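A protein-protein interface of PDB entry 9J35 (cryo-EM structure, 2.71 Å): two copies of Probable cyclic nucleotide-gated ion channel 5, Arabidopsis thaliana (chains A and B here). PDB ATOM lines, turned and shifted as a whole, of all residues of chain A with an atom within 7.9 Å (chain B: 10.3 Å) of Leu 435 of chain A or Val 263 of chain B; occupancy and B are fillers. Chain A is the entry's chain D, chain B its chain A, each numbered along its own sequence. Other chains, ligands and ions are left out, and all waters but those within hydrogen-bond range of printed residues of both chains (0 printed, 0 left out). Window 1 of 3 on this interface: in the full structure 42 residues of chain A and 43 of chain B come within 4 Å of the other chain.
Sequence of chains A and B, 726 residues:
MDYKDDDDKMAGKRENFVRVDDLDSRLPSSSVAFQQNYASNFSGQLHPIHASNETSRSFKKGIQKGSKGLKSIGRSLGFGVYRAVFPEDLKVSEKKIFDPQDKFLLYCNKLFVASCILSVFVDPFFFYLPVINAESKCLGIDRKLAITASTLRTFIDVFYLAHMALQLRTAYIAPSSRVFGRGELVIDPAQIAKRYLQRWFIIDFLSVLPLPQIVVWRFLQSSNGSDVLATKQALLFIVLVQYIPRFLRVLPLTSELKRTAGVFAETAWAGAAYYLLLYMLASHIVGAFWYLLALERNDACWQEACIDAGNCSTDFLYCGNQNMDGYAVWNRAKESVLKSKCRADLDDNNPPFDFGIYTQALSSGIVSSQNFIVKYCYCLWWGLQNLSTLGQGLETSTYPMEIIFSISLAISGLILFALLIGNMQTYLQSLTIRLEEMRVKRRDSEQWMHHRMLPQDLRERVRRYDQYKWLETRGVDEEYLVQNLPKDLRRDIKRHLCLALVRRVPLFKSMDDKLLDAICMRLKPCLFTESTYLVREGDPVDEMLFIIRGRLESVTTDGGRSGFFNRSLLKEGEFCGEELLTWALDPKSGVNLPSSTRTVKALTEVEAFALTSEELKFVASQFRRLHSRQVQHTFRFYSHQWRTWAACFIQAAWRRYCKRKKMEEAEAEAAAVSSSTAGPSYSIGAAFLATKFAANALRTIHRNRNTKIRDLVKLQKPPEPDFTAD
The side-chain hydroxyl (OG) of Ser 430 of chain B is in hydrogen-bond range of the side-chain carboxylate (OE1) of Glu 436 of chain A (3.3 Å).
OG1 of Thr 267 of chain B lies within hydrogen-bond range of NH1 of Arg 439 of chain A, 3.2 Å away.
NH2 of Arg 474 of chain A is in hydrogen-bond range of O of Arg 259 of chain B, at 2.9 Å.
Among the printed residues, pairs that only touch across the chains: Arg 442 of chain A with Phe 264 of chain B, Arg 439 of chain A with Phe 264 of chain B, Arg 474 of chain A with Gly 262 of chain B, Leu 471 of chain A with Gly 262 of chain B, Val 440 of chain A with Ser 430 of chain B, Met 438 of chain A with Phe 264 of chain B, Leu 435 of chain A with Phe 264 of chain B, Arg 474 of chain A with Lys 258 of chain B, Leu 435 of chain A with Val 263 of chain B, Arg 474 of chain A with Val 263 of chain B, Leu 471 of chain A with Thr 260 of chain B and Trp 470 of chain A with Val 263 of chain B.
No position is printed for both chains.
NH2 of Arg 259 of chain B is in salt-bridge range of OE1 of Glu 256 of chain B (3.6 Å).
The side-chain carboxylate (OE2) of Glu 436 of chain A lies within salt-bridge range of the guanidinium group (NH1) of Arg 439 of chain A, 3.0 Å away.
Of the 16 printed residues of chain A, 9 touch a printed residue of chain B.
Hydrophobic or aromatic side chains of chain A within 4 Å of the printed part of chain B: Leu 435, Met 438, Val 440, Trp 470 and Leu 471.
Among the printed residues, 15 pairs touch across the chains.
No residue of chain B comes within 4 Å of Thr 432 of chain A.
Of chain B, only Val 263 and Phe 264 come within 4 Å of Leu 435 of chain A.
Of the printed residues of chain B, Met 438 of chain A touches Phe 264.
Of the printed residues of chain B, Val 440 of chain A touches Ser 430.
Of the printed residues of chain A, Arg 259 of chain B touches Arg 474 (2.9 Å).
Of chain A, only Leu 435, Trp 470 and Arg 474 come within 4 Å of Val 263 of chain B.
The nearest printed residue of chain A that does not touch Ser 430 of chain B is Arg 439 of chain A (5.1 Å).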
ATOM      1  N   LEU A 431     -10.590 -11.386  20.102  1.00  0.00           N
ATOM      2  CA  LEU A 431     -10.958 -10.467  21.155  1.00  0.00           C
ATOM      3  C   LEU A 431     -10.915  -9.015  20.713  1.00  0.00           C
ATOM      4  O   LEU A 431     -11.513  -8.166  21.372  1.00  0.00           O
ATOM      5  CB  LEU A 431     -10.022 -10.692  22.342  1.00  0.00           C
ATOM      6  CG  LEU A 431     -10.258 -10.125  23.730  1.00  0.00           C
ATOM      7  CD1 LEU A 431     -11.172 -11.024  24.493  1.00  0.00           C
ATOM      8  CD2 LEU A 431      -8.922  -9.996  24.402  1.00  0.00           C
ATOM      9  N   THR A 432     -10.219  -8.705  19.624  1.00  0.00           N
ATOM     10  CA  THR A 432     -10.136  -7.351  19.098  1.00  0.00           C
ATOM     11  C   THR A 432     -10.660  -7.236  17.674  1.00  0.00           C
ATOM     12  O   THR A 432     -10.188  -6.385  16.928  1.00  0.00           O
ATOM     13  CB  THR A 432      -8.693  -6.836  19.160  1.00  0.00           C
ATOM     14  OG1 THR A 432      -7.780  -7.862  18.752  1.00  0.00           O
ATOM     15  CG2 THR A 432      -8.340  -6.389  20.553  1.00  0.00           C
ATOM     16  N   ILE A 433     -11.654  -8.033  17.296  1.00  0.00           N
ATOM     17  CA  ILE A 433     -12.054  -8.148  15.897  1.00  0.00           C
ATOM     18  C   ILE A 433     -12.842  -6.918  15.431  1.00  0.00           C
ATOM     19  O   ILE A 433     -12.594  -6.376  14.343  1.00  0.00           O
ATOM     20  CB  ILE A 433     -12.814  -9.477  15.706  1.00  0.00           C
ATOM     21  CG1 ILE A 433     -13.365  -9.630  14.305  1.00  0.00           C
ATOM     22  CG2 ILE A 433     -13.901  -9.669  16.741  1.00  0.00           C
ATOM     23  CD1 ILE A 433     -13.800 -10.999  14.024  1.00  0.00           C
ATOM     24  N   ARG A 434     -13.733  -6.408  16.281  1.00  0.00           N
ATOM     25  CA  ARG A 434     -14.514  -5.221  15.983  1.00  0.00           C
ATOM     26  C   ARG A 434     -13.678  -3.962  15.934  1.00  0.00           C
ATOM     27  O   ARG A 434     -13.994  -3.065  15.157  1.00  0.00           O
ATOM     28  CB  ARG A 434     -15.619  -5.024  17.021  1.00  0.00           C
ATOM     29  CG  ARG A 434     -16.670  -6.095  17.084  1.00  0.00           C
ATOM     30  CD  ARG A 434     -17.611  -5.998  15.962  1.00  0.00           C
ATOM     31  NE  ARG A 434     -18.269  -7.265  15.702  1.00  0.00           N
ATOM     32  CZ  ARG A 434     -17.940  -8.088  14.721  1.00  0.00           C
ATOM     33  NH1 ARG A 434     -16.953  -7.778  13.908  1.00  0.00           N
ATOM     34  NH2 ARG A 434     -18.588  -9.218  14.560  1.00  0.00           N
ATOM     35  N   LEU A 435     -12.629  -3.878  16.737  1.00  0.00           N
ATOM     36  CA  LEU A 435     -11.732  -2.735  16.741  1.00  0.00           C
ATOM     37  C   LEU A 435     -10.785  -2.734  15.558  1.00  0.00           C
ATOM     38  O   LEU A 435     -10.478  -1.669  15.028  1.00  0.00           O
ATOM     39  CB  LEU A 435     -10.935  -2.704  18.048  1.00  0.00           C
ATOM     40  CG  LEU A 435      -9.797  -1.685  18.214  1.00  0.00           C
ATOM     41  CD1 LEU A 435     -10.294  -0.351  18.721  1.00  0.00           C
ATOM     42  CD2 LEU A 435      -8.713  -2.213  19.098  1.00  0.00           C
ATOM     43  N   GLU A 436     -10.326  -3.896  15.121  1.00  0.00           N
ATOM     44  CA  GLU A 436      -9.536  -4.002  13.910  1.00  0.00           C
ATOM     45  C   GLU A 436     -10.328  -3.714  12.647  1.00  0.00           C
ATOM     46  O   GLU A 436      -9.733  -3.283  11.665  1.00  0.00           O
ATOM     47  CB  GLU A 436      -8.920  -5.391  13.795  1.00  0.00           C
ATOM     48  CG  GLU A 436      -7.827  -5.677  14.771  1.00  0.00           C
ATOM     49  CD  GLU A 436      -6.806  -4.576  14.877  1.00  0.00           C
ATOM     50  OE1 GLU A 436      -6.148  -4.263  13.872  1.00  0.00           O
ATOM     51  OE2 GLU A 436      -6.650  -4.022  15.980  1.00  0.00           O
ATOM     52  N   GLU A 437     -11.638  -3.928  12.645  1.00  0.00           N
ATOM     53  CA  GLU A 437     -12.443  -3.540  11.492  1.00  0.00           C
ATOM     54  C   GLU A 437     -12.588  -2.036  11.312  1.00  0.00           C
ATOM     55  O   GLU A 437     -12.588  -1.548  10.174  1.00  0.00           O
ATOM     56  CB  GLU A 437     -13.830  -4.136  11.609  1.00  0.00           C
ATOM     57  CG  GLU A 437     -13.868  -5.578  11.381  1.00  0.00           C
ATOM     58  CD  GLU A 437     -15.260  -6.092  11.447  1.00  0.00           C
ATOM     59  OE1 GLU A 437     -15.446  -7.309  11.661  1.00  0.00           O
ATOM     60  OE2 GLU A 437     -16.180  -5.266  11.285  1.00  0.00           O
ATOM     61  N   MET A 438     -12.720  -1.305  12.413  1.00  0.00           N
ATOM     62  CA  MET A 438     -12.814   0.145  12.419  1.00  0.00           C
ATOM     63  C   MET A 438     -11.546   0.806  11.882  1.00  0.00           C
ATOM     64  O   MET A 438     -11.617   1.809  11.159  1.00  0.00           O
ATOM     65  CB  MET A 438     -13.131   0.576  13.854  1.00  0.00           C
ATOM     66  CG  MET A 438     -13.613   1.986  14.063  1.00  0.00           C
ATOM     67  SD  MET A 438     -12.263   3.095  14.457  1.00  0.00           S
ATOM     68  CE  MET A 438     -11.645   2.336  15.935  1.00  0.00           C
ATOM     69  N   ARG A 439     -10.391   0.233  12.180  1.00  0.00           N
ATOM     70  CA  ARG A 439      -9.129   0.757  11.691  1.00  0.00           C
ATOM     71  C   ARG A 439      -8.915   0.502  10.208  1.00  0.00           C
ATOM     72  O   ARG A 439      -8.229   1.280   9.552  1.00  0.00           O
ATOM     73  CB  ARG A 439      -7.984   0.149  12.489  1.00  0.00           C
ATOM     74  CG  ARG A 439      -7.901   0.636  13.911  1.00  0.00           C
ATOM     75  CD  ARG A 439      -6.981  -0.233  14.706  1.00  0.00           C
ATOM     76  NE  ARG A 439      -6.802   0.265  16.058  1.00  0.00           N
ATOM     77  CZ  ARG A 439      -6.020  -0.303  16.966  1.00  0.00           C
ATOM     78  NH1 ARG A 439      -5.347  -1.397  16.670  1.00  0.00           N
ATOM     79  NH2 ARG A 439      -5.911   0.228  18.171  1.00  0.00           N
ATOM     80  N   VAL A 440      -9.479  -0.575   9.665  1.00  0.00           N
ATOM     81  CA  VAL A 440      -9.416  -0.829   8.231  1.00  0.00           C
ATOM     82  C   VAL A 440     -10.342   0.123   7.483  1.00  0.00           C
ATOM     83  O   VAL A 440      -9.987   0.661   6.423  1.00  0.00           O
ATOM     84  CB  VAL A 440      -9.745  -2.316   7.965  1.00  0.00           C
ATOM     85  CG1 VAL A 440      -9.999  -2.591   6.513  1.00  0.00           C
ATOM     86  CG2 VAL A 440      -8.624  -3.188   8.431  1.00  0.00           C
ATOM     87  N   LYS A 441     -11.519   0.389   8.060  1.00  0.00           N
ATOM     88  CA  LYS A 441     -12.485   1.306   7.469  1.00  0.00           C
ATOM     89  C   LYS A 441     -11.978   2.747   7.404  1.00  0.00           C
ATOM     90  O   LYS A 441     -12.233   3.452   6.417  1.00  0.00           O
ATOM     91  CB  LYS A 441     -13.783   1.209   8.261  1.00  0.00           C
ATOM     92  CG  LYS A 441     -14.875   2.155   7.861  1.00  0.00           C
ATOM     93  CD  LYS A 441     -16.189   1.735   8.451  1.00  0.00           C
ATOM     94  CE  LYS A 441     -17.212   2.861   8.449  1.00  0.00           C
ATOM     95  NZ  LYS A 441     -17.276   3.567   9.738  1.00  0.00           N
ATOM     96  N   ARG A 442     -11.224   3.192   8.409  1.00  0.00           N
ATOM     97  CA  ARG A 442     -10.673   4.545   8.360  1.00  0.00           C
ATOM     98  C   ARG A 442      -9.555   4.731   7.347  1.00  0.00           C
ATOM     99  O   ARG A 442      -9.487   5.783   6.705  1.00  0.00           O
ATOM    100  CB  ARG A 442     -10.166   4.949   9.722  1.00  0.00           C
ATOM    101  CG  ARG A 442     -11.246   5.252  10.682  1.00  0.00           C
ATOM    102  CD  ARG A 442     -10.639   5.820  11.898  1.00  0.00           C
ATOM    103  NE  ARG A 442      -9.399   5.125  12.181  1.00  0.00           N
ATOM    104  CZ  ARG A 442      -8.669   5.311  13.267  1.00  0.00           C
ATOM    105  NH1 ARG A 442      -9.062   6.171  14.194  1.00  0.00           N
ATOM    106  NH2 ARG A 442      -7.550   4.623  13.416  1.00  0.00           N
ATOM    107  N   TRP A 470     -18.930   5.038  15.849  1.00  0.00           N
ATOM    108  CA  TRP A 470     -18.122   4.114  16.639  1.00  0.00           C
ATOM    109  C   TRP A 470     -18.350   4.256  18.137  1.00  0.00           C
ATOM    110  O   TRP A 470     -18.354   3.249  18.847  1.00  0.00           O
ATOM    111  CB  TRP A 470     -16.634   4.287  16.334  1.00  0.00           C
ATOM    112  CG  TRP A 470     -15.711   3.490  17.248  1.00  0.00           C
ATOM    113  CD1 TRP A 470     -14.831   3.994  18.148  1.00  0.00           C
ATOM    114  CD2 TRP A 470     -15.591   2.063  17.342  1.00  0.00           C
ATOM    115  NE1 TRP A 470     -14.182   2.990  18.798  1.00  0.00           N
ATOM    116  CE2 TRP A 470     -14.626   1.791  18.318  1.00  0.00           C
ATOM    117  CE3 TRP A 470     -16.200   0.995  16.692  1.00  0.00           C
ATOM    118  CZ2 TRP A 470     -14.262   0.495  18.663  1.00  0.00           C
ATOM    119  CZ3 TRP A 470     -15.829  -0.275  17.025  1.00  0.00           C
ATOM    120  CH2 TRP A 470     -14.873  -0.520  18.002  1.00  0.00           C
ATOM    121  N   LEU A 471     -18.538   5.474  18.646  1.00  0.00           N
ATOM    122  CA  LEU A 471     -18.859   5.599  20.063  1.00  0.00           C
ATOM    123  C   LEU A 471     -20.256   5.108  20.408  1.00  0.00           C
ATOM    124  O   LEU A 471     -20.475   4.665  21.531  1.00  0.00           O
ATOM    125  CB  LEU A 471     -18.724   7.040  20.525  1.00  0.00           C
ATOM    126  CG  LEU A 471     -17.333   7.645  20.602  1.00  0.00           C
ATOM    127  CD1 LEU A 471     -17.413   8.870  21.436  1.00  0.00           C
ATOM    128  CD2 LEU A 471     -16.345   6.683  21.185  1.00  0.00           C
ATOM    129  N   ARG A 474     -20.189   0.532  18.794  1.00  0.00           N
ATOM    130  CA  ARG A 474     -19.017  -0.360  18.856  1.00  0.00           C
ATOM    131  C   ARG A 474     -18.981  -1.397  17.733  1.00  0.00           C
ATOM    132  O   ARG A 474     -18.501  -2.507  17.928  1.00  0.00           O
ATOM    133  CB  ARG A 474     -18.895  -1.074  20.201  1.00  0.00           C
ATOM    134  CG  ARG A 474     -19.164  -0.238  21.391  1.00  0.00           C
ATOM    135  CD  ARG A 474     -17.957   0.553  21.710  1.00  0.00           C
ATOM    136  NE  ARG A 474     -18.280   1.661  22.585  1.00  0.00           N
ATOM    137  CZ  ARG A 474     -17.405   2.589  22.919  1.00  0.00           C
ATOM    138  NH1 ARG A 474     -16.179   2.515  22.429  1.00  0.00           N
ATOM    139  NH2 ARG A 474     -17.746   3.579  23.728  1.00  0.00           N
ATOM    140  N   GLY A 475     -19.462  -1.053  16.549  1.00  0.00           N
ATOM    141  CA  GLY A 475     -19.405  -1.956  15.428  1.00  0.00           C
ATOM    142  C   GLY A 475     -20.436  -3.055  15.406  1.00  0.00           C
ATOM    143  O   GLY A 475     -20.348  -3.935  14.553  1.00  0.00           O
ATOM    144  N   THR B 254     -10.547   1.485  34.175  1.00  0.00           N
ATOM    145  CA  THR B 254     -10.301   1.260  32.756  1.00  0.00           C
ATOM    146  C   THR B 254     -11.595   1.036  31.983  1.00  0.00           C
ATOM    147  O   THR B 254     -11.711   1.487  30.838  1.00  0.00           O
ATOM    148  CB  THR B 254      -9.353   0.084  32.564  1.00  0.00           C
ATOM    149  OG1 THR B 254      -9.806  -1.025  33.345  1.00  0.00           O
ATOM    150  CG2 THR B 254      -7.967   0.470  33.004  1.00  0.00           C
ATOM    151  N   SER B 255     -12.583   0.379  32.596  1.00  0.00           N
ATOM    152  CA  SER B 255     -13.883   0.215  31.954  1.00  0.00           C
ATOM    153  C   SER B 255     -14.616   1.541  31.817  1.00  0.00           C
ATOM    154  O   SER B 255     -15.458   1.692  30.930  1.00  0.00           O
ATOM    155  CB  SER B 255     -14.746  -0.771  32.735  1.00  0.00           C
ATOM    156  OG  SER B 255     -15.169  -0.213  33.962  1.00  0.00           O
ATOM    157  N   GLU B 256     -14.327   2.506  32.683  1.00  0.00           N
ATOM    158  CA  GLU B 256     -14.928   3.818  32.484  1.00  0.00           C
ATOM    159  C   GLU B 256     -14.166   4.693  31.499  1.00  0.00           C
ATOM    160  O   GLU B 256     -14.656   5.771  31.158  1.00  0.00           O
ATOM    161  CB  GLU B 256     -15.090   4.540  33.816  1.00  0.00           C
ATOM    162  CG  GLU B 256     -16.026   3.791  34.720  1.00  0.00           C
ATOM    163  CD  GLU B 256     -17.385   3.598  34.075  1.00  0.00           C
ATOM    164  OE1 GLU B 256     -17.986   4.599  33.641  1.00  0.00           O
ATOM    165  OE2 GLU B 256     -17.838   2.443  33.975  1.00  0.00           O
ATOM    166  N   LEU B 257     -12.997   4.274  31.034  1.00  0.00           N
ATOM    167  CA  LEU B 257     -12.362   4.912  29.891  1.00  0.00           C
ATOM    168  C   LEU B 257     -12.618   4.153  28.597  1.00  0.00           C
ATOM    169  O   LEU B 257     -12.355   4.688  27.518  1.00  0.00           O
ATOM    170  CB  LEU B 257     -10.854   5.062  30.116  1.00  0.00           C
ATOM    171  CG  LEU B 257     -10.320   6.342  30.769  1.00  0.00           C
ATOM    172  CD1 LEU B 257     -10.643   6.423  32.252  1.00  0.00           C
ATOM    173  CD2 LEU B 257      -8.821   6.450  30.558  1.00  0.00           C
ATOM    174  N   LYS B 258     -13.134   2.923  28.683  1.00  0.00           N
ATOM    175  CA  LYS B 258     -13.592   2.173  27.518  1.00  0.00           C
ATOM    176  C   LYS B 258     -15.007   2.547  27.088  1.00  0.00           C
ATOM    177  O   LYS B 258     -15.649   1.767  26.380  1.00  0.00           O
ATOM    178  CB  LYS B 258     -13.557   0.665  27.781  1.00  0.00           C
ATOM    179  CG  LYS B 258     -12.198   0.020  27.995  1.00  0.00           C
ATOM    180  CD  LYS B 258     -11.363  -0.113  26.741  1.00  0.00           C
ATOM    181  CE  LYS B 258     -10.093  -0.895  27.067  1.00  0.00           C
ATOM    182  NZ  LYS B 258      -9.177  -1.073  25.910  1.00  0.00           N
ATOM    183  N   ARG B 259     -15.520   3.704  27.506  1.00  0.00           N
ATOM    184  CA  ARG B 259     -16.890   4.086  27.187  1.00  0.00           C
ATOM    185  C   ARG B 259     -17.040   5.474  26.589  1.00  0.00           C
ATOM    186  O   ARG B 259     -17.954   5.675  25.780  1.00  0.00           O
ATOM    187  CB  ARG B 259     -17.771   4.010  28.436  1.00  0.00           C
ATOM    188  CG  ARG B 259     -18.454   2.679  28.645  1.00  0.00           C
ATOM    189  CD  ARG B 259     -19.242   2.688  29.943  1.00  0.00           C
ATOM    190  NE  ARG B 259     -19.712   4.029  30.287  1.00  0.00           N
ATOM    191  CZ  ARG B 259     -20.536   4.301  31.293  1.00  0.00           C
ATOM    192  NH1 ARG B 259     -20.910   5.549  31.529  1.00  0.00           N
ATOM    193  NH2 ARG B 259     -20.989   3.323  32.064  1.00  0.00           N
ATOM    194  N   THR B 260     -16.192   6.432  26.946  1.00  0.00           N
ATOM    195  CA  THR B 260     -16.340   7.801  26.477  1.00  0.00           C
ATOM    196  C   THR B 260     -15.276   8.217  25.479  1.00  0.00           C
ATOM    197  O   THR B 260     -15.433   9.249  24.827  1.00  0.00           O
ATOM    198  CB  THR B 260     -16.297   8.777  27.656  1.00  0.00           C
ATOM    199  OG1 THR B 260     -14.935   8.971  28.053  1.00  0.00           O
ATOM    200  CG2 THR B 260     -17.102   8.239  28.838  1.00  0.00           C
ATOM    201  N   ALA B 261     -14.195   7.453  25.357  1.00  0.00           N
ATOM    202  CA  ALA B 261     -13.110   7.786  24.446  1.00  0.00           C
ATOM    203  C   ALA B 261     -12.822   6.642  23.485  1.00  0.00           C
ATOM    204  O   ALA B 261     -11.759   6.607  22.861  1.00  0.00           O
ATOM    205  CB  ALA B 261     -11.850   8.163  25.227  1.00  0.00           C
ATOM    206  N   GLY B 262     -13.753   5.713  23.361  1.00  0.00           N
ATOM    207  CA  GLY B 262     -13.572   4.599  22.453  1.00  0.00           C
ATOM    208  C   GLY B 262     -12.647   3.568  23.048  1.00  0.00           C
ATOM    209  O   GLY B 262     -12.395   3.542  24.261  1.00  0.00           O
ATOM    210  N   VAL B 263     -12.125   2.698  22.191  1.00  0.00           N
ATOM    211  CA  VAL B 263     -11.173   1.686  22.622  1.00  0.00           C
ATOM    212  C   VAL B 263      -9.866   2.029  21.919  1.00  0.00           C
ATOM    213  O   VAL B 263      -8.776   1.658  22.370  1.00  0.00           O
ATOM    214  CB  VAL B 263     -11.684   0.268  22.288  1.00  0.00           C
ATOM    215  CG1 VAL B 263     -10.810  -0.805  22.914  1.00  0.00           C
ATOM    216  CG2 VAL B 263     -13.139   0.099  22.706  1.00  0.00           C
ATOM    217  N   PHE B 264      -9.972   2.785  20.827  1.00  0.00           N
ATOM    218  CA  PHE B 264      -8.821   3.162  20.005  1.00  0.00           C
ATOM    219  C   PHE B 264      -8.093   4.318  20.663  1.00  0.00           C
ATOM    220  O   PHE B 264      -8.665   5.382  20.906  1.00  0.00           O
ATOM    221  CB  PHE B 264      -9.256   3.551  18.598  1.00  0.00           C
ATOM    222  CG  PHE B 264      -8.137   4.085  17.748  1.00  0.00           C
ATOM    223  CD1 PHE B 264      -7.180   3.235  17.241  1.00  0.00           C
ATOM    224  CD2 PHE B 264      -8.036   5.436  17.466  1.00  0.00           C
ATOM    225  CE1 PHE B 264      -6.149   3.714  16.459  1.00  0.00           C
ATOM    226  CE2 PHE B 264      -6.995   5.917  16.692  1.00  0.00           C
ATOM    227  CZ  PHE B 264      -6.055   5.053  16.193  1.00  0.00           C
ATOM    228  N   ALA B 265      -6.811   4.115  20.960  1.00  0.00           N
ATOM    229  CA  ALA B 265      -5.939   5.254  21.215  1.00  0.00           C
ATOM    230  C   ALA B 265      -5.069   5.544  19.997  1.00  0.00           C
ATOM    231  O   ALA B 265      -5.134   6.630  19.412  1.00  0.00           O
ATOM    232  CB  ALA B 265      -5.089   4.997  22.458  1.00  0.00           C
ATOM    233  N   GLU B 266      -4.271   4.559  19.589  1.00  0.00           N
ATOM    234  CA  GLU B 266      -3.297   4.637  18.504  1.00  0.00           C
ATOM    235  C   GLU B 266      -2.800   3.218  18.282  1.00  0.00           C
ATOM    236  O   GLU B 266      -2.707   2.428  19.222  1.00  0.00           O
ATOM    237  CB  GLU B 266      -2.136   5.578  18.846  1.00  0.00           C
ATOM    238  CG  GLU B 266      -1.158   5.863  17.719  1.00  0.00           C
ATOM    239  CD  GLU B 266      -1.757   6.711  16.627  1.00  0.00           C
ATOM    240  OE1 GLU B 266      -2.707   7.466  16.914  1.00  0.00           O
ATOM    241  OE2 GLU B 266      -1.268   6.644  15.486  1.00  0.00           O
ATOM    242  N   THR B 267      -2.478   2.893  17.035  1.00  0.00           N
ATOM    243  CA  THR B 267      -2.068   1.529  16.730  1.00  0.00           C
ATOM    244  C   THR B 267      -0.587   1.385  16.386  1.00  0.00           C
ATOM    245  O   THR B 267      -0.024   0.304  16.570  1.00  0.00           O
ATOM    246  CB  THR B 267      -2.936   0.961  15.600  1.00  0.00           C
ATOM    247  OG1 THR B 267      -2.580  -0.402  15.362  1.00  0.00           O
ATOM    248  CG2 THR B 267      -2.806   1.761  14.324  1.00  0.00           C
ATOM    249  N   ALA B 270       1.476   3.392  19.567  1.00  0.00           N
ATOM    250  CA  ALA B 270       1.043   2.747  20.793  1.00  0.00           C
ATOM    251  C   ALA B 270       0.579   1.343  20.417  1.00  0.00           C
ATOM    252  O   ALA B 270       0.791   0.899  19.283  1.00  0.00           O
ATOM    253  CB  ALA B 270      -0.048   3.576  21.490  1.00  0.00           C
ATOM    254  N   GLY B 271      -0.043   0.640  21.361  1.00  0.00           N
ATOM    255  CA  GLY B 271      -0.629  -0.654  21.074  1.00  0.00           C
ATOM    256  C   GLY B 271       0.335  -1.823  21.114  1.00  0.00           C
ATOM    257  O   GLY B 271       0.122  -2.786  21.856  1.00  0.00           O
ATOM    258  N   ALA B 272       1.381  -1.775  20.296  1.00  0.00           N
ATOM    259  CA  ALA B 272       2.466  -2.742  20.376  1.00  0.00           C
ATOM    260  C   ALA B 272       3.637  -2.207  21.179  1.00  0.00           C
ATOM    261  O   ALA B 272       4.520  -2.979  21.558  1.00  0.00           O
ATOM    262  CB  ALA B 272       2.928  -3.150  18.975  1.00  0.00           C
ATOM    263  N   ASN B 423       0.297  -9.999  19.358  1.00  0.00           N
ATOM    264  CA  ASN B 423      -0.230  -8.671  19.085  1.00  0.00           C
ATOM    265  C   ASN B 423       0.446  -7.967  17.937  1.00  0.00           C
ATOM    266  O   ASN B 423      -0.177  -7.102  17.418  1.00  0.00           O
ATOM    267  CB  ASN B 423      -0.034  -7.889  20.351  1.00  0.00           C
ATOM    268  CG  ASN B 423      -1.163  -8.054  21.343  1.00  0.00           C
ATOM    269  OD1 ASN B 423      -1.166  -8.991  22.127  1.00  0.00           O
ATOM    270  ND2 ASN B 423      -2.112  -7.135  21.328  1.00  0.00           N
ATOM    271  N   THR B 426      -1.274  -9.627  14.830  1.00  0.00           N
ATOM    272  CA  THR B 426      -2.571  -9.063  14.462  1.00  0.00           C
ATOM    273  C   THR B 426      -2.463  -7.634  13.958  1.00  0.00           C
ATOM    274  O   THR B 426      -3.288  -7.218  13.146  1.00  0.00           O
ATOM    275  CB  THR B 426      -3.587  -9.081  15.609  1.00  0.00           C
ATOM    276  OG1 THR B 426      -3.252  -8.095  16.580  1.00  0.00           O
ATOM    277  CG2 THR B 426      -3.690 -10.420  16.252  1.00  0.00           C
ATOM    278  N   TYR B 427      -1.469  -6.874  14.414  1.00  0.00           N
ATOM    279  CA  TYR B 427      -1.275  -5.537  13.874  1.00  0.00           C
ATOM    280  C   TYR B 427      -0.799  -5.577  12.427  1.00  0.00           C
ATOM    281  O   TYR B 427      -1.249  -4.776  11.605  1.00  0.00           O
ATOM    282  CB  TYR B 427      -0.296  -4.759  14.743  1.00  0.00           C
ATOM    283  CG  TYR B 427       0.232  -3.505  14.092  1.00  0.00           C
ATOM    284  CD1 TYR B 427      -0.539  -2.363  14.033  1.00  0.00           C
ATOM    285  CD2 TYR B 427       1.506  -3.461  13.543  1.00  0.00           C
ATOM    286  CE1 TYR B 427      -0.074  -1.224  13.439  1.00  0.00           C
ATOM    287  CE2 TYR B 427       1.967  -2.340  12.940  1.00  0.00           C
ATOM    288  CZ  TYR B 427       1.180  -1.225  12.897  1.00  0.00           C
ATOM    289  OH  TYR B 427       1.663  -0.093  12.300  1.00  0.00           O
ATOM    290  N   SER B 430      -3.555  -6.770   9.675  1.00  0.00           N
ATOM    291  CA  SER B 430      -4.566  -5.768   9.409  1.00  0.00           C
ATOM    292  C   SER B 430      -4.060  -4.623   8.548  1.00  0.00           C
ATOM    293  O   SER B 430      -4.852  -3.801   8.100  1.00  0.00           O
ATOM    294  CB  SER B 430      -5.087  -5.235  10.738  1.00  0.00           C
ATOM    295  OG  SER B 430      -5.972  -4.161  10.573  1.00  0.00           O
